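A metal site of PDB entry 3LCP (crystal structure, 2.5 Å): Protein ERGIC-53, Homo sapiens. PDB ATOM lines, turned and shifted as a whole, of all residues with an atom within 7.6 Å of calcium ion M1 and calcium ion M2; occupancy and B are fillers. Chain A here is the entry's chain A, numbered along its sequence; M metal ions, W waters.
Water W2 lies within hydrogen-bond range of the backbone carbonyl oxygen of Asn 131 (2.7 Å) and the side-chain amide nitrogen of Asn 132 (3.3 Å). Water W4 lies within hydrogen-bond range of the side-chain amide nitrogen of Asn 131 (2.6 Å) and the side-chain carboxylate of Asp 127 (2.8 Å). Water W1 bridges the side-chain hydroxyl (OH) of Tyr 146 (2.6 Å) and the backbone carbonyl oxygen (O) of His 148 (3.2 Å).
Calcium ion M2 is bound by OD2 of Asp 151 (2.1 Å). Water W3 is bound to calcium ion M2, at 2.3 Å. The side-chain amide oxygen (OD1) of Asn 126 is bound to calcium ion M2 (2.4 Å). Calcium ion M2 is bound by water W1 (2.5 Å). Calcium ion M2 is bound by O of Phe 124, 2.5 Å away. OD2 of Asp 122 is bound to calcium ion M2, 2.6 Å away. Calcium ion M2 is bound by OD1 of Asp 122 (2.7 Å).
Merely in contact with calcium ion M2: His 148. Within 4 Å of calcium ion M2: Asp 122, Phe 124, Asn 126, His 148 and Asp 151. The nearest printed residue that does not touch calcium ion M2 is Asn 132 (4.7 Å).
The side-chain carboxylate (OD2) of Asp 125 lies within hydrogen-bond range of the backbone NH (N) of Lys 130 (2.7 Å). The backbone NH (N) of Asp 122 lies within hydrogen-bond range of the backbone carbonyl oxygen (O) of Ala 134 (2.6 Å). O of Gln 149 is in hydrogen-bond range of N of Asp 127, 3.3 Å away. The side-chain carboxylate (OD2) of Asp 125 lies within hydrogen-bond range of the backbone NH (N) of Lys 129 (3.4 Å). The side-chain amide nitrogen (ND2) of Asn 132 sits at hydrogen-bond distance from the backbone carbonyl oxygen (O) of Asp 122 (3.3 Å). The side-chain amide nitrogen (NE2) of Gln 161 sits at hydrogen-bond distance from the backbone carbonyl oxygen (O) of Asn 131 (2.9 Å). ND2 of Asn 132 sits close to O of Phe 124, 3.1 Å away. The backbone NH (N) of Gly 128 lies close to the side-chain carboxylate (OD1) of Asp 125 (3.1 Å).
Five residues have an atom within 4 Å of calcium ion M1: Asp 125, Asp 127, Asn 131, Asn 132 and Asp 151. The nearest printed residue that does not touch calcium ion M1 is Lys 129 (4.3 Å).
Calcium ion M1 is bound by OD1 of Asn 131 (2.2 Å), OD1 of Asp 151 (2.2 Å), water W4 (2.3 Å), OD1 of Asn 132 (2.4 Å), OD1 of Asp 127 (2.5 Å), OD1 of Asp 125 (2.5 Å) and water W2 (2.7 Å). Calcium ion M1 has seven donor atoms within binding distance.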
ATOM      1  N   ASP A  91     -14.897 -18.539  -8.539  1.00  0.00           N
ATOM      2  CA  ASP A  91     -14.889 -18.543 -10.003  1.00  0.00           C
ATOM      3  C   ASP A  91     -14.155 -19.729 -10.536  1.00  0.00           C
ATOM      4  O   ASP A  91     -14.534 -20.300 -11.573  1.00  0.00           O
ATOM      5  CB  ASP A  91     -14.152 -17.286 -10.522  1.00  0.00           C
ATOM      6  CG  ASP A  91     -15.079 -16.082 -10.630  1.00  0.00           C
ATOM      7  OD1 ASP A  91     -16.171 -16.229 -11.209  1.00  0.00           O
ATOM      8  OD2 ASP A  91     -14.714 -15.009 -10.118  1.00  0.00           O
ATOM      9  N   GLY A  92     -13.043 -20.062  -9.858  1.00  0.00           N
ATOM     10  CA  GLY A  92     -12.314 -21.293 -10.137  1.00  0.00           C
ATOM     11  C   GLY A  92     -10.836 -21.171  -9.901  1.00  0.00           C
ATOM     12  O   GLY A  92     -10.355 -20.207  -9.300  1.00  0.00           O
ATOM     13  N   PHE A 108      -8.559 -15.567 -13.356  1.00  0.00           N
ATOM     14  CA  PHE A 108      -8.623 -16.482 -12.237  1.00  0.00           C
ATOM     15  C   PHE A 108      -7.584 -16.147 -11.201  1.00  0.00           C
ATOM     16  O   PHE A 108      -6.933 -17.061 -10.660  1.00  0.00           O
ATOM     17  CB  PHE A 108      -8.443 -17.949 -12.691  1.00  0.00           C
ATOM     18  CG  PHE A 108      -9.610 -18.491 -13.412  1.00  0.00           C
ATOM     19  CD1 PHE A 108     -10.622 -19.146 -12.709  1.00  0.00           C
ATOM     20  CD2 PHE A 108      -9.748 -18.322 -14.790  1.00  0.00           C
ATOM     21  CE1 PHE A 108     -11.732 -19.630 -13.359  1.00  0.00           C
ATOM     22  CE2 PHE A 108     -10.840 -18.817 -15.453  1.00  0.00           C
ATOM     23  CZ  PHE A 108     -11.841 -19.466 -14.731  1.00  0.00           C
ATOM     24  N   PHE A 121      -9.751 -24.497 -14.284  1.00  0.00           N
ATOM     25  CA  PHE A 121     -10.738 -25.312 -13.672  1.00  0.00           C
ATOM     26  C   PHE A 121     -11.906 -24.350 -13.389  1.00  0.00           C
ATOM     27  O   PHE A 121     -11.895 -23.630 -12.378  1.00  0.00           O
ATOM     28  CB  PHE A 121     -10.126 -25.948 -12.406  1.00  0.00           C
ATOM     29  CG  PHE A 121      -9.038 -26.927 -12.718  1.00  0.00           C
ATOM     30  CD1 PHE A 121      -7.800 -26.490 -13.103  1.00  0.00           C
ATOM     31  CD2 PHE A 121      -9.279 -28.283 -12.655  1.00  0.00           C
ATOM     32  CE1 PHE A 121      -6.778 -27.370 -13.399  1.00  0.00           C
ATOM     33  CE2 PHE A 121      -8.302 -29.192 -12.975  1.00  0.00           C
ATOM     34  CZ  PHE A 121      -7.011 -28.707 -13.347  1.00  0.00           C
ATOM     35  N   ASP A 122     -12.858 -24.314 -14.324  1.00  0.00           N
ATOM     36  CA  ASP A 122     -13.859 -23.238 -14.369  1.00  0.00           C
ATOM     37  C   ASP A 122     -15.166 -23.738 -13.751  1.00  0.00           C
ATOM     38  O   ASP A 122     -15.869 -24.569 -14.305  1.00  0.00           O
ATOM     39  CB  ASP A 122     -14.098 -22.745 -15.801  1.00  0.00           C
ATOM     40  CG  ASP A 122     -14.804 -21.377 -15.871  1.00  0.00           C
ATOM     41  OD1 ASP A 122     -14.481 -20.590 -16.769  1.00  0.00           O
ATOM     42  OD2 ASP A 122     -15.688 -21.071 -15.056  1.00  0.00           O
ATOM     43  N   SER A 123     -15.447 -23.234 -12.576  1.00  0.00           N
ATOM     44  CA  SER A 123     -16.669 -23.667 -11.901  1.00  0.00           C
ATOM     45  C   SER A 123     -17.855 -22.750 -12.210  1.00  0.00           C
ATOM     46  O   SER A 123     -18.991 -23.141 -12.001  1.00  0.00           O
ATOM     47  CB  SER A 123     -16.412 -23.786 -10.398  1.00  0.00           C
ATOM     48  OG  SER A 123     -16.008 -22.539  -9.885  1.00  0.00           O
ATOM     49  N   PHE A 124     -17.598 -21.556 -12.776  1.00  0.00           N
ATOM     50  CA  PHE A 124     -18.722 -20.613 -13.033  1.00  0.00           C
ATOM     51  C   PHE A 124     -19.143 -20.391 -14.496  1.00  0.00           C
ATOM     52  O   PHE A 124     -18.329 -20.046 -15.347  1.00  0.00           O
ATOM     53  CB  PHE A 124     -18.537 -19.289 -12.301  1.00  0.00           C
ATOM     54  CG  PHE A 124     -19.766 -18.410 -12.331  1.00  0.00           C
ATOM     55  CD1 PHE A 124     -20.864 -18.716 -11.544  1.00  0.00           C
ATOM     56  CD2 PHE A 124     -19.810 -17.298 -13.158  1.00  0.00           C
ATOM     57  CE1 PHE A 124     -22.011 -17.901 -11.573  1.00  0.00           C
ATOM     58  CE2 PHE A 124     -20.945 -16.473 -13.219  1.00  0.00           C
ATOM     59  CZ  PHE A 124     -22.047 -16.770 -12.422  1.00  0.00           C
ATOM     60  N   ASP A 125     -20.428 -20.620 -14.766  1.00  0.00           N
ATOM     61  CA  ASP A 125     -20.974 -20.688 -16.115  1.00  0.00           C
ATOM     62  C   ASP A 125     -21.300 -19.259 -16.589  1.00  0.00           C
ATOM     63  O   ASP A 125     -22.408 -18.737 -16.415  1.00  0.00           O
ATOM     64  CB  ASP A 125     -22.202 -21.639 -16.123  1.00  0.00           C
ATOM     65  CG  ASP A 125     -22.763 -21.886 -17.516  1.00  0.00           C
ATOM     66  OD1 ASP A 125     -22.141 -21.494 -18.525  1.00  0.00           O
ATOM     67  OD2 ASP A 125     -23.827 -22.533 -17.624  1.00  0.00           O
ATOM     68  N   ASN A 126     -20.316 -18.585 -17.137  1.00  0.00           N
ATOM     69  CA  ASN A 126     -20.496 -17.180 -17.398  1.00  0.00           C
ATOM     70  C   ASN A 126     -21.332 -16.933 -18.626  1.00  0.00           C
ATOM     71  O   ASN A 126     -22.045 -15.950 -18.666  1.00  0.00           O
ATOM     72  CB  ASN A 126     -19.153 -16.460 -17.471  1.00  0.00           C
ATOM     73  CG  ASN A 126     -18.612 -16.176 -16.126  1.00  0.00           C
ATOM     74  OD1 ASN A 126     -17.804 -16.944 -15.579  1.00  0.00           O
ATOM     75  ND2 ASN A 126     -19.059 -15.074 -15.548  1.00  0.00           N
ATOM     76  N   ASP A 127     -21.248 -17.833 -19.605  1.00  0.00           N
ATOM     77  CA  ASP A 127     -22.035 -17.747 -20.845  1.00  0.00           C
ATOM     78  C   ASP A 127     -23.363 -18.551 -20.823  1.00  0.00           C
ATOM     79  O   ASP A 127     -24.036 -18.691 -21.872  1.00  0.00           O
ATOM     80  CB  ASP A 127     -21.177 -18.202 -22.047  1.00  0.00           C
ATOM     81  CG  ASP A 127     -20.589 -19.601 -21.840  1.00  0.00           C
ATOM     82  OD1 ASP A 127     -20.858 -20.239 -20.781  1.00  0.00           O
ATOM     83  OD2 ASP A 127     -19.883 -20.096 -22.759  1.00  0.00           O
ATOM     84  N   GLY A 128     -23.743 -19.078 -19.652  1.00  0.00           N
ATOM     85  CA  GLY A 128     -25.015 -19.792 -19.488  1.00  0.00           C
ATOM     86  C   GLY A 128     -25.234 -20.967 -20.411  1.00  0.00           C
ATOM     87  O   GLY A 128     -26.381 -21.329 -20.726  1.00  0.00           O
ATOM     88  N   LYS A 129     -24.134 -21.587 -20.854  1.00  0.00           N
ATOM     89  CA  LYS A 129     -24.210 -22.736 -21.766  1.00  0.00           C
ATOM     90  C   LYS A 129     -24.431 -24.073 -21.060  1.00  0.00           C
ATOM     91  O   LYS A 129     -24.425 -25.124 -21.703  1.00  0.00           O
ATOM     92  CB  LYS A 129     -22.967 -22.798 -22.664  1.00  0.00           C
ATOM     93  CG  LYS A 129     -22.957 -21.729 -23.749  1.00  0.00           C
ATOM     94  CD  LYS A 129     -22.555 -22.320 -25.100  1.00  0.00           C
ATOM     95  CE  LYS A 129     -23.376 -21.691 -26.238  1.00  0.00           C
ATOM     96  NZ  LYS A 129     -23.418 -20.196 -26.216  1.00  0.00           N
ATOM     97  N   LYS A 130     -24.623 -24.030 -19.734  1.00  0.00           N
ATOM     98  CA  LYS A 130     -24.894 -25.238 -18.914  1.00  0.00           C
ATOM     99  C   LYS A 130     -23.744 -26.265 -18.961  1.00  0.00           C
ATOM    100  O   LYS A 130     -23.986 -27.495 -18.962  1.00  0.00           O
ATOM    101  CB  LYS A 130     -26.227 -25.931 -19.308  1.00  0.00           C
ATOM    102  CG  LYS A 130     -27.472 -25.037 -19.538  1.00  0.00           C
ATOM    103  CD  LYS A 130     -28.234 -24.753 -18.254  1.00  0.00           C
ATOM    104  CE  LYS A 130     -29.558 -24.101 -18.590  1.00  0.00           C
ATOM    105  NZ  LYS A 130     -30.527 -24.097 -17.453  1.00  0.00           N
ATOM    106  N   ASN A 131     -22.500 -25.772 -19.035  1.00  0.00           N
ATOM    107  CA  ASN A 131     -21.340 -26.631 -19.289  1.00  0.00           C
ATOM    108  C   ASN A 131     -20.197 -26.367 -18.305  1.00  0.00           C
ATOM    109  O   ASN A 131     -19.045 -26.111 -18.715  1.00  0.00           O
ATOM    110  CB  ASN A 131     -20.892 -26.560 -20.762  1.00  0.00           C
ATOM    111  CG  ASN A 131     -20.443 -25.143 -21.217  1.00  0.00           C
ATOM    112  OD1 ASN A 131     -20.661 -24.133 -20.536  1.00  0.00           O
ATOM    113  ND2 ASN A 131     -19.793 -25.086 -22.383  1.00  0.00           N
ATOM    114  N   ASN A 132     -20.545 -26.428 -17.028  1.00  0.00           N
ATOM    115  CA  ASN A 132     -19.665 -26.162 -15.898  1.00  0.00           C
ATOM    116  C   ASN A 132     -20.130 -27.018 -14.708  1.00  0.00           C
ATOM    117  O   ASN A 132     -21.285 -27.457 -14.687  1.00  0.00           O
ATOM    118  CB  ASN A 132     -19.743 -24.707 -15.478  1.00  0.00           C
ATOM    119  CG  ASN A 132     -19.220 -23.746 -16.527  1.00  0.00           C
ATOM    120  OD1 ASN A 132     -19.813 -23.585 -17.603  1.00  0.00           O
ATOM    121  ND2 ASN A 132     -18.145 -23.033 -16.191  1.00  0.00           N
ATOM    122  N   ALA A 134     -16.095 -26.962 -15.502  1.00  0.00           N
ATOM    123  CA  ALA A 134     -15.368 -27.436 -16.686  1.00  0.00           C
ATOM    124  C   ALA A 134     -13.900 -27.208 -16.511  1.00  0.00           C
ATOM    125  O   ALA A 134     -13.516 -26.334 -15.745  1.00  0.00           O
ATOM    126  CB  ALA A 134     -15.838 -26.702 -17.943  1.00  0.00           C
ATOM    127  N   TYR A 146      -7.868 -13.039 -22.221  1.00  0.00           N
ATOM    128  CA  TYR A 146      -8.803 -14.086 -21.782  1.00  0.00           C
ATOM    129  C   TYR A 146     -10.258 -13.625 -21.914  1.00  0.00           C
ATOM    130  O   TYR A 146     -10.639 -12.559 -21.404  1.00  0.00           O
ATOM    131  CB  TYR A 146      -8.517 -14.522 -20.347  1.00  0.00           C
ATOM    132  CG  TYR A 146      -9.519 -15.524 -19.818  1.00  0.00           C
ATOM    133  CD1 TYR A 146      -9.627 -16.781 -20.381  1.00  0.00           C
ATOM    134  CD2 TYR A 146     -10.339 -15.218 -18.729  1.00  0.00           C
ATOM    135  CE1 TYR A 146     -10.535 -17.702 -19.907  1.00  0.00           C
ATOM    136  CE2 TYR A 146     -11.258 -16.135 -18.234  1.00  0.00           C
ATOM    137  CZ  TYR A 146     -11.353 -17.368 -18.839  1.00  0.00           C
ATOM    138  OH  TYR A 146     -12.239 -18.308 -18.398  1.00  0.00           O
ATOM    139  N   ASP A 147     -11.058 -14.402 -22.618  1.00  0.00           N
ATOM    140  CA  ASP A 147     -12.467 -14.097 -22.682  1.00  0.00           C
ATOM    141  C   ASP A 147     -13.241 -14.810 -21.565  1.00  0.00           C
ATOM    142  O   ASP A 147     -13.677 -15.943 -21.754  1.00  0.00           O
ATOM    143  CB  ASP A 147     -13.009 -14.490 -24.054  1.00  0.00           C
ATOM    144  CG  ASP A 147     -14.479 -14.122 -24.233  1.00  0.00           C
ATOM    145  OD1 ASP A 147     -15.193 -14.864 -24.939  1.00  0.00           O
ATOM    146  OD2 ASP A 147     -14.928 -13.107 -23.672  1.00  0.00           O
ATOM    147  N   HIS A 148     -13.414 -14.167 -20.417  1.00  0.00           N
ATOM    148  CA  HIS A 148     -14.065 -14.857 -19.276  1.00  0.00           C
ATOM    149  C   HIS A 148     -15.568 -14.910 -19.350  1.00  0.00           C
ATOM    150  O   HIS A 148     -16.166 -15.706 -18.607  1.00  0.00           O
ATOM    151  CB  HIS A 148     -13.644 -14.320 -17.861  1.00  0.00           C
ATOM    152  CG  HIS A 148     -13.849 -12.849 -17.727  1.00  0.00           C
ATOM    153  ND1 HIS A 148     -14.408 -12.153 -18.769  1.00  0.00           N
ATOM    154  CD2 HIS A 148     -13.429 -11.784 -16.888  1.00  0.00           C
ATOM    155  CE1 HIS A 148     -14.453 -10.816 -18.612  1.00  0.00           C
ATOM    156  NE2 HIS A 148     -13.789 -10.515 -17.516  1.00  0.00           N
ATOM    157  N   GLN A 149     -16.183 -14.096 -20.206  1.00  0.00           N
ATOM    158  CA  GLN A 149     -17.637 -14.073 -20.338  1.00  0.00           C
ATOM    159  C   GLN A 149     -18.126 -15.248 -21.165  1.00  0.00           C
ATOM    160  O   GLN A 149     -19.303 -15.608 -21.092  1.00  0.00           O
ATOM    161  CB  GLN A 149     -18.121 -12.746 -20.940  1.00  0.00           C
ATOM    162  CG  GLN A 149     -17.937 -11.522 -20.024  1.00  0.00           C
ATOM    163  CD  GLN A 149     -18.595 -11.696 -18.632  1.00  0.00           C
ATOM    164  OE1 GLN A 149     -17.966 -11.427 -17.601  1.00  0.00           O
ATOM    165  NE2 GLN A 149     -19.853 -12.110 -18.609  1.00  0.00           N
ATOM    166  N   ASN A 150     -17.237 -15.846 -21.934  1.00  0.00           N
ATOM    167  CA  ASN A 150     -17.561 -17.099 -22.599  1.00  0.00           C
ATOM    168  C   ASN A 150     -16.777 -18.287 -22.059  1.00  0.00           C
ATOM    169  O   ASN A 150     -16.616 -19.288 -22.743  1.00  0.00           O
ATOM    170  CB  ASN A 150     -17.385 -16.983 -24.107  1.00  0.00           C
ATOM    171  CG  ASN A 150     -18.573 -16.299 -24.794  1.00  0.00           C
ATOM    172  OD1 ASN A 150     -19.641 -16.058 -24.195  1.00  0.00           O
ATOM    173  ND2 ASN A 150     -18.379 -15.967 -26.068  1.00  0.00           N
ATOM    174  N   ASP A 151     -16.279 -18.159 -20.826  1.00  0.00           N
ATOM    175  CA  ASP A 151     -15.514 -19.246 -20.175  1.00  0.00           C
ATOM    176  C   ASP A 151     -14.415 -19.772 -21.094  1.00  0.00           C
ATOM    177  O   ASP A 151     -14.165 -20.974 -21.140  1.00  0.00           O
ATOM    178  CB  ASP A 151     -16.442 -20.414 -19.855  1.00  0.00           C
ATOM    179  CG  ASP A 151     -17.468 -20.102 -18.799  1.00  0.00           C
ATOM    180  OD1 ASP A 151     -18.519 -20.738 -18.938  1.00  0.00           O
ATOM    181  OD2 ASP A 151     -17.215 -19.333 -17.831  1.00  0.00           O
ATOM    182  N   GLY A 152     -13.839 -18.866 -21.877  1.00  0.00           N
ATOM    183  CA  GLY A 152     -12.739 -19.148 -22.792  1.00  0.00           C
ATOM    184  C   GLY A 152     -13.068 -20.042 -23.949  1.00  0.00           C
ATOM    185  O   GLY A 152     -12.172 -20.454 -24.693  1.00  0.00           O
ATOM    186  N   ALA A 153     -14.358 -20.317 -24.146  1.00  0.00           N
ATOM    187  CA  ALA A 153     -14.804 -21.174 -25.248  1.00  0.00           C
ATOM    188  C   ALA A 153     -14.343 -20.757 -26.650  1.00  0.00           C
ATOM    189  O   ALA A 153     -14.324 -21.571 -27.572  1.00  0.00           O
ATOM    190  CB  ALA A 153     -16.296 -21.324 -25.220  1.00  0.00           C
ATOM    191  N   GLN A 161     -15.628 -31.820 -19.114  1.00  0.00           N
ATOM    192  CA  GLN A 161     -16.592 -31.562 -18.065  1.00  0.00           C
ATOM    193  C   GLN A 161     -16.239 -32.401 -16.851  1.00  0.00           C
ATOM    194  O   GLN A 161     -16.449 -33.594 -16.876  1.00  0.00           O
ATOM    195  CB  GLN A 161     -18.006 -31.915 -18.557  1.00  0.00           C
ATOM    196  CG  GLN A 161     -18.459 -31.096 -19.797  1.00  0.00           C
ATOM    197  CD  GLN A 161     -19.049 -29.763 -19.417  1.00  0.00           C
ATOM    198  OE1 GLN A 161     -20.111 -29.702 -18.805  1.00  0.00           O
ATOM    199  NE2 GLN A 161     -18.356 -28.684 -19.755  1.00  0.00           N
HETATM  200 CA    CA M   1     -19.990 -22.240 -19.628  1.00  0.00          CA
HETATM  201 CA    CA M   2     -16.313 -18.704 -16.067  1.00  0.00          CA
HETATM  202  O   HOH W   1     -14.240 -17.579 -16.941  1.00  0.00           O
HETATM  203  O   HOH W   2     -17.799 -23.847 -19.325  1.00  0.00           O
HETATM  204  O   HOH W   3     -15.525 -18.448 -13.937  1.00  0.00           O
HETATM  205  O   HOH W   4     -19.095 -22.642 -21.755  1.00  0.00           O
